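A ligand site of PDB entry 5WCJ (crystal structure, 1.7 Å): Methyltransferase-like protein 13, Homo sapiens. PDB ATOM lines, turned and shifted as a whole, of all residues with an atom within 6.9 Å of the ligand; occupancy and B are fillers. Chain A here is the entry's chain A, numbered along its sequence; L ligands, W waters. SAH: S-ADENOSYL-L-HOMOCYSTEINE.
An oxygen (O2') of the ligand is in hydrogen-bond range of the side-chain carboxylate (OE2) of Glu 73.
A nitrogen (N6) of the ligand lies within hydrogen-bond range of the side-chain carboxylate of Asp 100, at 2.9 Å.
A nitrogen (N1) of the ligand sits at hydrogen-bond distance from the backbone NH of Gly 101, 3.0 Å away.
The backbone NH (N) of Gly 52 is in hydrogen-bond range of an oxygen (O3') of the ligand, 3.1 Å away.
The backbone NH (N) of Ile 74 is in hydrogen-bond range of a nitrogen (N3) of the ligand, at 3.3 Å.
N of Leu 51 is in hydrogen-bond range of OE1 of Glu 73 (2.8 Å).
The backbone NH (N) of Ala 99 lies within hydrogen-bond range of the backbone carbonyl oxygen (O) of Glu 73, at 3.0 Å.
The backbone NH (N) of Asp 75 is in hydrogen-bond range of the side-chain carboxylate (OE2) of Glu 73 (3.0 Å).
The side-chain carboxylate (OD1) of Asp 100 lies within hydrogen-bond range of the backbone NH (N) of Leu 102, at 3.1 Å.
The backbone carbonyl oxygen (O) of Ala 99 sits close to the backbone NH (N) of Ile 74, at 3.3 Å.
OD2 of Asp 124 lies within hydrogen-bond range of NE2 of His 23, at 2.7 Å.
OD1 of Asp 124 is in hydrogen-bond range of NE2 of His 22 (3.1 Å).
OD1 of Asp 124 lies within hydrogen-bond range of ND2 of Asn 163 (3.2 Å).
Merely in contact with the ligand: Val 49 (3.7 Å), Gly 50 (3.5 Å), Leu 51 (3.8 Å), Asp 75 (3.9 Å), Met 78 (3.6 Å), Ala 99 (3.8 Å), Asp 124 (3.5 Å), Val 125 (3.3 Å), Asp 126 (3.5 Å) and Phe 141 (3.5 Å).
Hydrophobic or aromatic side chains within 4 Å of the ligand: Val 49, Ile 74, Met 78, Val 125 and Phe 141.
Within 4 Å of the ligand: Val 49, Gly 50, Leu 51, Gly 52, Glu 73, Ile 74, Asp 75, Met 78, Ala 99, Asp 100, Gly 101, Asp 124, Val 125, Asp 126 and Phe 141.
The nearest printed residue that does not touch the ligand is Val 72 (4.03 Å).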
ATOM      1  N   HIS A  22      20.939  33.029  39.029  1.00  0.00           N
ATOM      2  CA  HIS A  22      19.535  32.767  38.704  1.00  0.00           C
ATOM      3  C   HIS A  22      19.117  31.367  39.144  1.00  0.00           C
ATOM      4  O   HIS A  22      17.973  31.174  39.559  1.00  0.00           O
ATOM      5  CB  HIS A  22      19.158  33.134  37.262  1.00  0.00           C
ATOM      6  CG  HIS A  22      19.429  32.073  36.241  1.00  0.00           C
ATOM      7  ND1 HIS A  22      20.604  32.018  35.529  1.00  0.00           N
ATOM      8  CD2 HIS A  22      18.637  31.088  35.744  1.00  0.00           C
ATOM      9  CE1 HIS A  22      20.541  31.007  34.676  1.00  0.00           C
ATOM     10  NE2 HIS A  22      19.365  30.432  34.787  1.00  0.00           N
ATOM     11  N   HIS A  23      20.050  30.410  39.142  1.00  0.00           N
ATOM     12  CA  HIS A  23      19.733  29.078  39.694  1.00  0.00           C
ATOM     13  C   HIS A  23      19.445  29.090  41.179  1.00  0.00           C
ATOM     14  O   HIS A  23      18.478  28.469  41.625  1.00  0.00           O
ATOM     15  CB  HIS A  23      20.806  28.058  39.338  1.00  0.00           C
ATOM     16  CG  HIS A  23      20.755  27.631  37.902  1.00  0.00           C
ATOM     17  ND1 HIS A  23      21.819  27.028  37.264  1.00  0.00           N
ATOM     18  CD2 HIS A  23      19.767  27.732  36.975  1.00  0.00           C
ATOM     19  CE1 HIS A  23      21.481  26.756  36.018  1.00  0.00           C
ATOM     20  NE2 HIS A  23      20.252  27.189  35.804  1.00  0.00           N
ATOM     21  N   VAL A  49      12.549  21.908  32.621  1.00  0.00           N
ATOM     22  CA  VAL A  49      12.712  22.032  31.187  1.00  0.00           C
ATOM     23  C   VAL A  49      13.891  22.918  30.933  1.00  0.00           C
ATOM     24  O   VAL A  49      13.908  24.086  31.383  1.00  0.00           O
ATOM     25  CB  VAL A  49      11.470  22.648  30.523  1.00  0.00           C
ATOM     26  CG1 VAL A  49      11.650  22.652  29.018  1.00  0.00           C
ATOM     27  CG2 VAL A  49      10.232  21.873  30.951  1.00  0.00           C
ATOM     28  N   GLY A  50      14.867  22.365  30.210  1.00  0.00           N
ATOM     29  CA  GLY A  50      16.099  23.031  29.880  1.00  0.00           C
ATOM     30  C   GLY A  50      17.195  22.519  30.785  1.00  0.00           C
ATOM     31  O   GLY A  50      17.158  22.772  31.980  1.00  0.00           O
ATOM     32  N   LEU A  51      18.160  21.783  30.225  1.00  0.00           N
ATOM     33  CA  LEU A  51      19.261  21.172  31.044  1.00  0.00           C
ATOM     34  C   LEU A  51      20.424  22.116  31.300  1.00  0.00           C
ATOM     35  O   LEU A  51      21.002  22.086  32.395  1.00  0.00           O
ATOM     36  CB  LEU A  51      19.789  19.907  30.369  1.00  0.00           C
ATOM     37  CG  LEU A  51      20.805  19.054  31.148  1.00  0.00           C
ATOM     38  CD1 LEU A  51      20.142  18.435  32.366  1.00  0.00           C
ATOM     39  CD2 LEU A  51      21.379  17.986  30.218  1.00  0.00           C
ATOM     40  N   GLY A  52      20.789  22.904  30.286  1.00  0.00           N
ATOM     41  CA  GLY A  52      22.056  23.634  30.268  1.00  0.00           C
ATOM     42  C   GLY A  52      23.197  22.672  30.548  1.00  0.00           C
ATOM     43  O   GLY A  52      23.217  21.549  30.035  1.00  0.00           O
ATOM     44  N   GLY A  53      24.115  23.098  31.409  1.00  0.00           N
ATOM     45  CA  GLY A  53      25.200  22.243  31.884  1.00  0.00           C
ATOM     46  C   GLY A  53      24.794  21.181  32.907  1.00  0.00           C
ATOM     47  O   GLY A  53      25.644  20.390  33.310  1.00  0.00           O
ATOM     48  N   VAL A  72      13.710  17.703  30.858  1.00  0.00           N
ATOM     49  CA  VAL A  72      13.437  17.660  29.425  1.00  0.00           C
ATOM     50  C   VAL A  72      14.388  18.604  28.697  1.00  0.00           C
ATOM     51  O   VAL A  72      14.538  19.749  29.080  1.00  0.00           O
ATOM     52  CB  VAL A  72      11.968  18.023  29.150  1.00  0.00           C
ATOM     53  CG1 VAL A  72      11.672  17.916  27.662  1.00  0.00           C
ATOM     54  CG2 VAL A  72      11.064  17.138  29.972  1.00  0.00           C
ATOM     55  N   GLU A  73      15.092  18.111  27.687  1.00  0.00           N
ATOM     56  CA  GLU A  73      16.121  18.868  27.012  1.00  0.00           C
ATOM     57  C   GLU A  73      15.989  18.618  25.510  1.00  0.00           C
ATOM     58  O   GLU A  73      15.929  17.472  25.089  1.00  0.00           O
ATOM     59  CB  GLU A  73      17.507  18.418  27.509  1.00  0.00           C
ATOM     60  CG  GLU A  73      18.695  18.932  26.714  1.00  0.00           C
ATOM     61  CD  GLU A  73      18.696  20.435  26.533  1.00  0.00           C
ATOM     62  OE1 GLU A  73      18.482  21.174  27.536  1.00  0.00           O
ATOM     63  OE2 GLU A  73      18.941  20.907  25.381  1.00  0.00           O
ATOM     64  N   ILE A  74      15.967  19.680  24.722  1.00  0.00           N
ATOM     65  CA  ILE A  74      15.714  19.543  23.265  1.00  0.00           C
ATOM     66  C   ILE A  74      16.945  19.055  22.478  1.00  0.00           C
ATOM     67  O   ILE A  74      16.785  18.376  21.463  1.00  0.00           O
ATOM     68  CB  ILE A  74      15.188  20.860  22.655  1.00  0.00           C
ATOM     69  CG1 ILE A  74      14.485  20.611  21.327  1.00  0.00           C
ATOM     70  CG2 ILE A  74      16.267  21.907  22.518  1.00  0.00           C
ATOM     71  CD1 ILE A  74      13.825  21.882  20.797  1.00  0.00           C
ATOM     72  N   ASP A  75      18.150  19.347  22.988  1.00  0.00           N
ATOM     73  CA  ASP A  75      19.412  19.172  22.252  1.00  0.00           C
ATOM     74  C   ASP A  75      20.201  18.020  22.872  1.00  0.00           C
ATOM     75  O   ASP A  75      20.723  18.170  23.994  1.00  0.00           O
ATOM     76  CB  ASP A  75      20.212  20.466  22.316  1.00  0.00           C
ATOM     77  CG  ASP A  75      21.526  20.436  21.517  1.00  0.00           C
ATOM     78  OD1 ASP A  75      21.896  19.380  20.954  1.00  0.00           O
ATOM     79  OD2 ASP A  75      22.200  21.487  21.482  1.00  0.00           O
ATOM     80  N   MET A  78      23.644  18.698  24.472  1.00  0.00           N
ATOM     81  CA  MET A  78      23.735  19.273  25.806  1.00  0.00           C
ATOM     82  C   MET A  78      23.802  18.179  26.861  1.00  0.00           C
ATOM     83  O   MET A  78      24.567  18.286  27.822  1.00  0.00           O
ATOM     84  CB  MET A  78      22.556  20.231  26.062  1.00  0.00           C
ATOM     85  CG  MET A  78      22.566  21.456  25.146  1.00  0.00           C
ATOM     86  SD  MET A  78      23.966  22.552  25.390  1.00  0.00           S
ATOM     87  CE  MET A  78      23.630  23.191  27.005  1.00  0.00           C
ATOM     88  N   LEU A  79      22.973  17.163  26.731  1.00  0.00           N
ATOM     89  CA  LEU A  79      23.042  16.002  27.626  1.00  0.00           C
ATOM     90  C   LEU A  79      24.386  15.279  27.506  1.00  0.00           C
ATOM     91  O   LEU A  79      24.948  14.864  28.523  1.00  0.00           O
ATOM     92  CB  LEU A  79      21.911  15.028  27.382  1.00  0.00           C
ATOM     93  CG  LEU A  79      21.904  13.708  28.194  1.00  0.00           C
ATOM     94  CD1 LEU A  79      21.797  14.004  29.682  1.00  0.00           C
ATOM     95  CD2 LEU A  79      20.789  12.772  27.762  1.00  0.00           C
ATOM     96  N   ALA A  99      13.587  15.922  24.062  1.00  0.00           N
ATOM     97  CA  ALA A  99      12.321  16.367  23.493  1.00  0.00           C
ATOM     98  C   ALA A  99      12.203  17.876  23.610  1.00  0.00           C
ATOM     99  O   ALA A  99      12.880  18.524  24.457  1.00  0.00           O
ATOM    100  CB  ALA A  99      11.143  15.696  24.199  1.00  0.00           C
ATOM    101  N   ASP A 100      11.383  18.462  22.755  1.00  0.00           N
ATOM    102  CA  ASP A 100      10.939  19.835  22.914  1.00  0.00           C
ATOM    103  C   ASP A 100      10.037  19.815  24.135  1.00  0.00           C
ATOM    104  O   ASP A 100       9.118  19.019  24.207  1.00  0.00           O
ATOM    105  CB  ASP A 100      10.152  20.252  21.666  1.00  0.00           C
ATOM    106  CG  ASP A 100       9.753  21.708  21.646  1.00  0.00           C
ATOM    107  OD1 ASP A 100       9.640  22.401  22.713  1.00  0.00           O
ATOM    108  OD2 ASP A 100       9.502  22.169  20.506  1.00  0.00           O
ATOM    109  N   GLY A 101      10.293  20.674  25.124  1.00  0.00           N
ATOM    110  CA  GLY A 101       9.424  20.749  26.324  1.00  0.00           C
ATOM    111  C   GLY A 101       7.931  20.995  26.002  1.00  0.00           C
ATOM    112  O   GLY A 101       7.070  20.549  26.729  1.00  0.00           O
ATOM    113  N   LEU A 102       7.650  21.732  24.929  1.00  0.00           N
ATOM    114  CA  LEU A 102       6.262  21.984  24.497  1.00  0.00           C
ATOM    115  C   LEU A 102       5.540  20.689  24.149  1.00  0.00           C
ATOM    116  O   LEU A 102       4.475  20.379  24.727  1.00  0.00           O
ATOM    117  CB  LEU A 102       6.230  22.955  23.338  1.00  0.00           C
ATOM    118  CG  LEU A 102       6.706  24.361  23.647  1.00  0.00           C
ATOM    119  CD1 LEU A 102       7.060  25.030  22.349  1.00  0.00           C
ATOM    120  CD2 LEU A 102       5.701  25.168  24.474  1.00  0.00           C
ATOM    121  N   ASP A 124      13.740  26.647  32.586  1.00  0.00           N
ATOM    122  CA  ASP A 124      15.055  27.257  32.443  1.00  0.00           C
ATOM    123  C   ASP A 124      15.430  27.100  30.979  1.00  0.00           C
ATOM    124  O   ASP A 124      16.472  26.521  30.646  1.00  0.00           O
ATOM    125  CB  ASP A 124      16.055  26.530  33.365  1.00  0.00           C
ATOM    126  CG  ASP A 124      17.359  27.264  33.561  1.00  0.00           C
ATOM    127  OD1 ASP A 124      17.415  28.485  33.351  1.00  0.00           O
ATOM    128  OD2 ASP A 124      18.369  26.577  33.967  1.00  0.00           O
ATOM    129  N   VAL A 125      14.545  27.551  30.117  1.00  0.00           N
ATOM    130  CA  VAL A 125      14.655  27.279  28.686  1.00  0.00           C
ATOM    131  C   VAL A 125      15.055  28.538  27.936  1.00  0.00           C
ATOM    132  O   VAL A 125      14.504  29.615  28.187  1.00  0.00           O
ATOM    133  CB  VAL A 125      13.402  26.555  28.139  1.00  0.00           C
ATOM    134  CG1 VAL A 125      12.124  27.208  28.587  1.00  0.00           C
ATOM    135  CG2 VAL A 125      13.448  26.435  26.634  1.00  0.00           C
ATOM    136  N   ASP A 126      16.063  28.428  27.078  1.00  0.00           N
ATOM    137  CA  ASP A 126      16.564  29.563  26.312  1.00  0.00           C
ATOM    138  C   ASP A 126      17.003  29.042  24.943  1.00  0.00           C
ATOM    139  O   ASP A 126      17.883  28.201  24.890  1.00  0.00           O
ATOM    140  CB  ASP A 126      17.728  30.233  27.038  1.00  0.00           C
ATOM    141  CG  ASP A 126      18.157  31.556  26.404  1.00  0.00           C
ATOM    142  OD1 ASP A 126      17.612  31.970  25.344  1.00  0.00           O
ATOM    143  OD2 ASP A 126      19.073  32.182  26.961  1.00  0.00           O
ATOM    144  N   SER A 127      16.357  29.512  23.873  1.00  0.00           N
ATOM    145  CA  SER A 127      16.713  29.055  22.515  1.00  0.00           C
ATOM    146  C   SER A 127      17.801  29.901  21.857  1.00  0.00           C
ATOM    147  O   SER A 127      18.282  30.881  22.425  1.00  0.00           O
ATOM    148  CB  SER A 127      15.476  29.051  21.632  1.00  0.00           C
ATOM    149  OG  SER A 127      14.960  30.353  21.543  1.00  0.00           O
ATOM    150  N   SER A 135      13.470  34.857  23.770  1.00  0.00           N
ATOM    151  CA  SER A 135      14.036  33.515  23.640  1.00  0.00           C
ATOM    152  C   SER A 135      14.139  32.750  24.977  1.00  0.00           C
ATOM    153  O   SER A 135      14.414  31.546  24.951  1.00  0.00           O
ATOM    154  CB  SER A 135      15.423  33.590  22.975  1.00  0.00           C
ATOM    155  OG  SER A 135      16.263  34.436  23.724  1.00  0.00           O
ATOM    156  N   PRO A 138      11.165  30.735  24.976  1.00  0.00           N
ATOM    157  CA  PRO A 138      10.390  30.975  23.757  1.00  0.00           C
ATOM    158  C   PRO A 138       8.912  31.285  24.088  1.00  0.00           C
ATOM    159  O   PRO A 138       8.356  30.709  25.031  1.00  0.00           O
ATOM    160  CB  PRO A 138      10.539  29.652  22.982  1.00  0.00           C
ATOM    161  CG  PRO A 138      11.813  29.061  23.506  1.00  0.00           C
ATOM    162  CD  PRO A 138      11.834  29.426  24.950  1.00  0.00           C
ATOM    163  N   PHE A 141       5.927  28.919  25.374  1.00  0.00           N
ATOM    164  CA  PHE A 141       5.931  28.345  26.721  1.00  0.00           C
ATOM    165  C   PHE A 141       5.084  29.151  27.691  1.00  0.00           C
ATOM    166  O   PHE A 141       4.740  28.658  28.752  1.00  0.00           O
ATOM    167  CB  PHE A 141       7.357  28.245  27.299  1.00  0.00           C
ATOM    168  CG  PHE A 141       8.156  27.097  26.777  1.00  0.00           C
ATOM    169  CD1 PHE A 141       8.918  27.217  25.640  1.00  0.00           C
ATOM    170  CD2 PHE A 141       8.116  25.863  27.426  1.00  0.00           C
ATOM    171  CE1 PHE A 141       9.677  26.155  25.162  1.00  0.00           C
ATOM    172  CE2 PHE A 141       8.852  24.779  26.964  1.00  0.00           C
ATOM    173  CZ  PHE A 141       9.646  24.922  25.831  1.00  0.00           C
ATOM    174  N   ASN A 163      12.340  31.216  34.554  1.00  0.00           N
ATOM    175  CA  ASN A 163      13.438  32.131  34.302  1.00  0.00           C
ATOM    176  C   ASN A 163      13.000  32.937  33.081  1.00  0.00           C
ATOM    177  O   ASN A 163      12.822  32.363  32.010  1.00  0.00           O
ATOM    178  CB  ASN A 163      14.714  31.353  34.020  1.00  0.00           C
ATOM    179  CG  ASN A 163      15.899  32.232  33.630  1.00  0.00           C
ATOM    180  OD1 ASN A 163      15.939  33.402  33.955  1.00  0.00           O
ATOM    181  ND2 ASN A 163      16.878  31.637  32.927  1.00  0.00           N
HETATM  182  CG  SAH L   1      19.944  26.932  30.719  1.00  0.00           C
HETATM  183  SD  SAH L   1      20.456  26.721  28.996  1.00  0.00           S
HETATM  184  C5' SAH L   1      18.878  26.610  28.101  1.00  0.00           C
HETATM  185  C4' SAH L   1      18.584  25.151  27.818  1.00  0.00           C
HETATM  186  O4' SAH L   1      17.270  25.060  27.219  1.00  0.00           O
HETATM  187  C3' SAH L   1      19.568  24.521  26.808  1.00  0.00           C
HETATM  188  O3' SAH L   1      20.009  23.255  27.292  1.00  0.00           O
HETATM  189  C2' SAH L   1      18.705  24.351  25.551  1.00  0.00           C
HETATM  190  O2' SAH L   1      19.040  23.264  24.695  1.00  0.00           O
HETATM  191  C1' SAH L   1      17.359  24.082  26.199  1.00  0.00           C
HETATM  192  N9  SAH L   1      16.202  24.258  25.332  1.00  0.00           N
HETATM  193  C8  SAH L   1      16.012  25.232  24.381  1.00  0.00           C
HETATM  194  N7  SAH L   1      14.831  25.193  23.805  1.00  0.00           N
HETATM  195  C5  SAH L   1      14.206  24.117  24.408  1.00  0.00           C
HETATM  196  C6  SAH L   1      12.926  23.551  24.260  1.00  0.00           C
HETATM  197  N6  SAH L   1      11.989  24.040  23.401  1.00  0.00           N
HETATM  198  N1  SAH L   1      12.626  22.481  25.007  1.00  0.00           N
HETATM  199  C2  SAH L   1      13.540  21.991  25.858  1.00  0.00           C
HETATM  200  N3  SAH L   1      14.778  22.448  26.096  1.00  0.00           N
HETATM  201  C4  SAH L   1      15.049  23.525  25.342  1.00  0.00           C
HETATM  202  O   HOH W   1      10.950  25.959  21.423  1.00  0.00           O
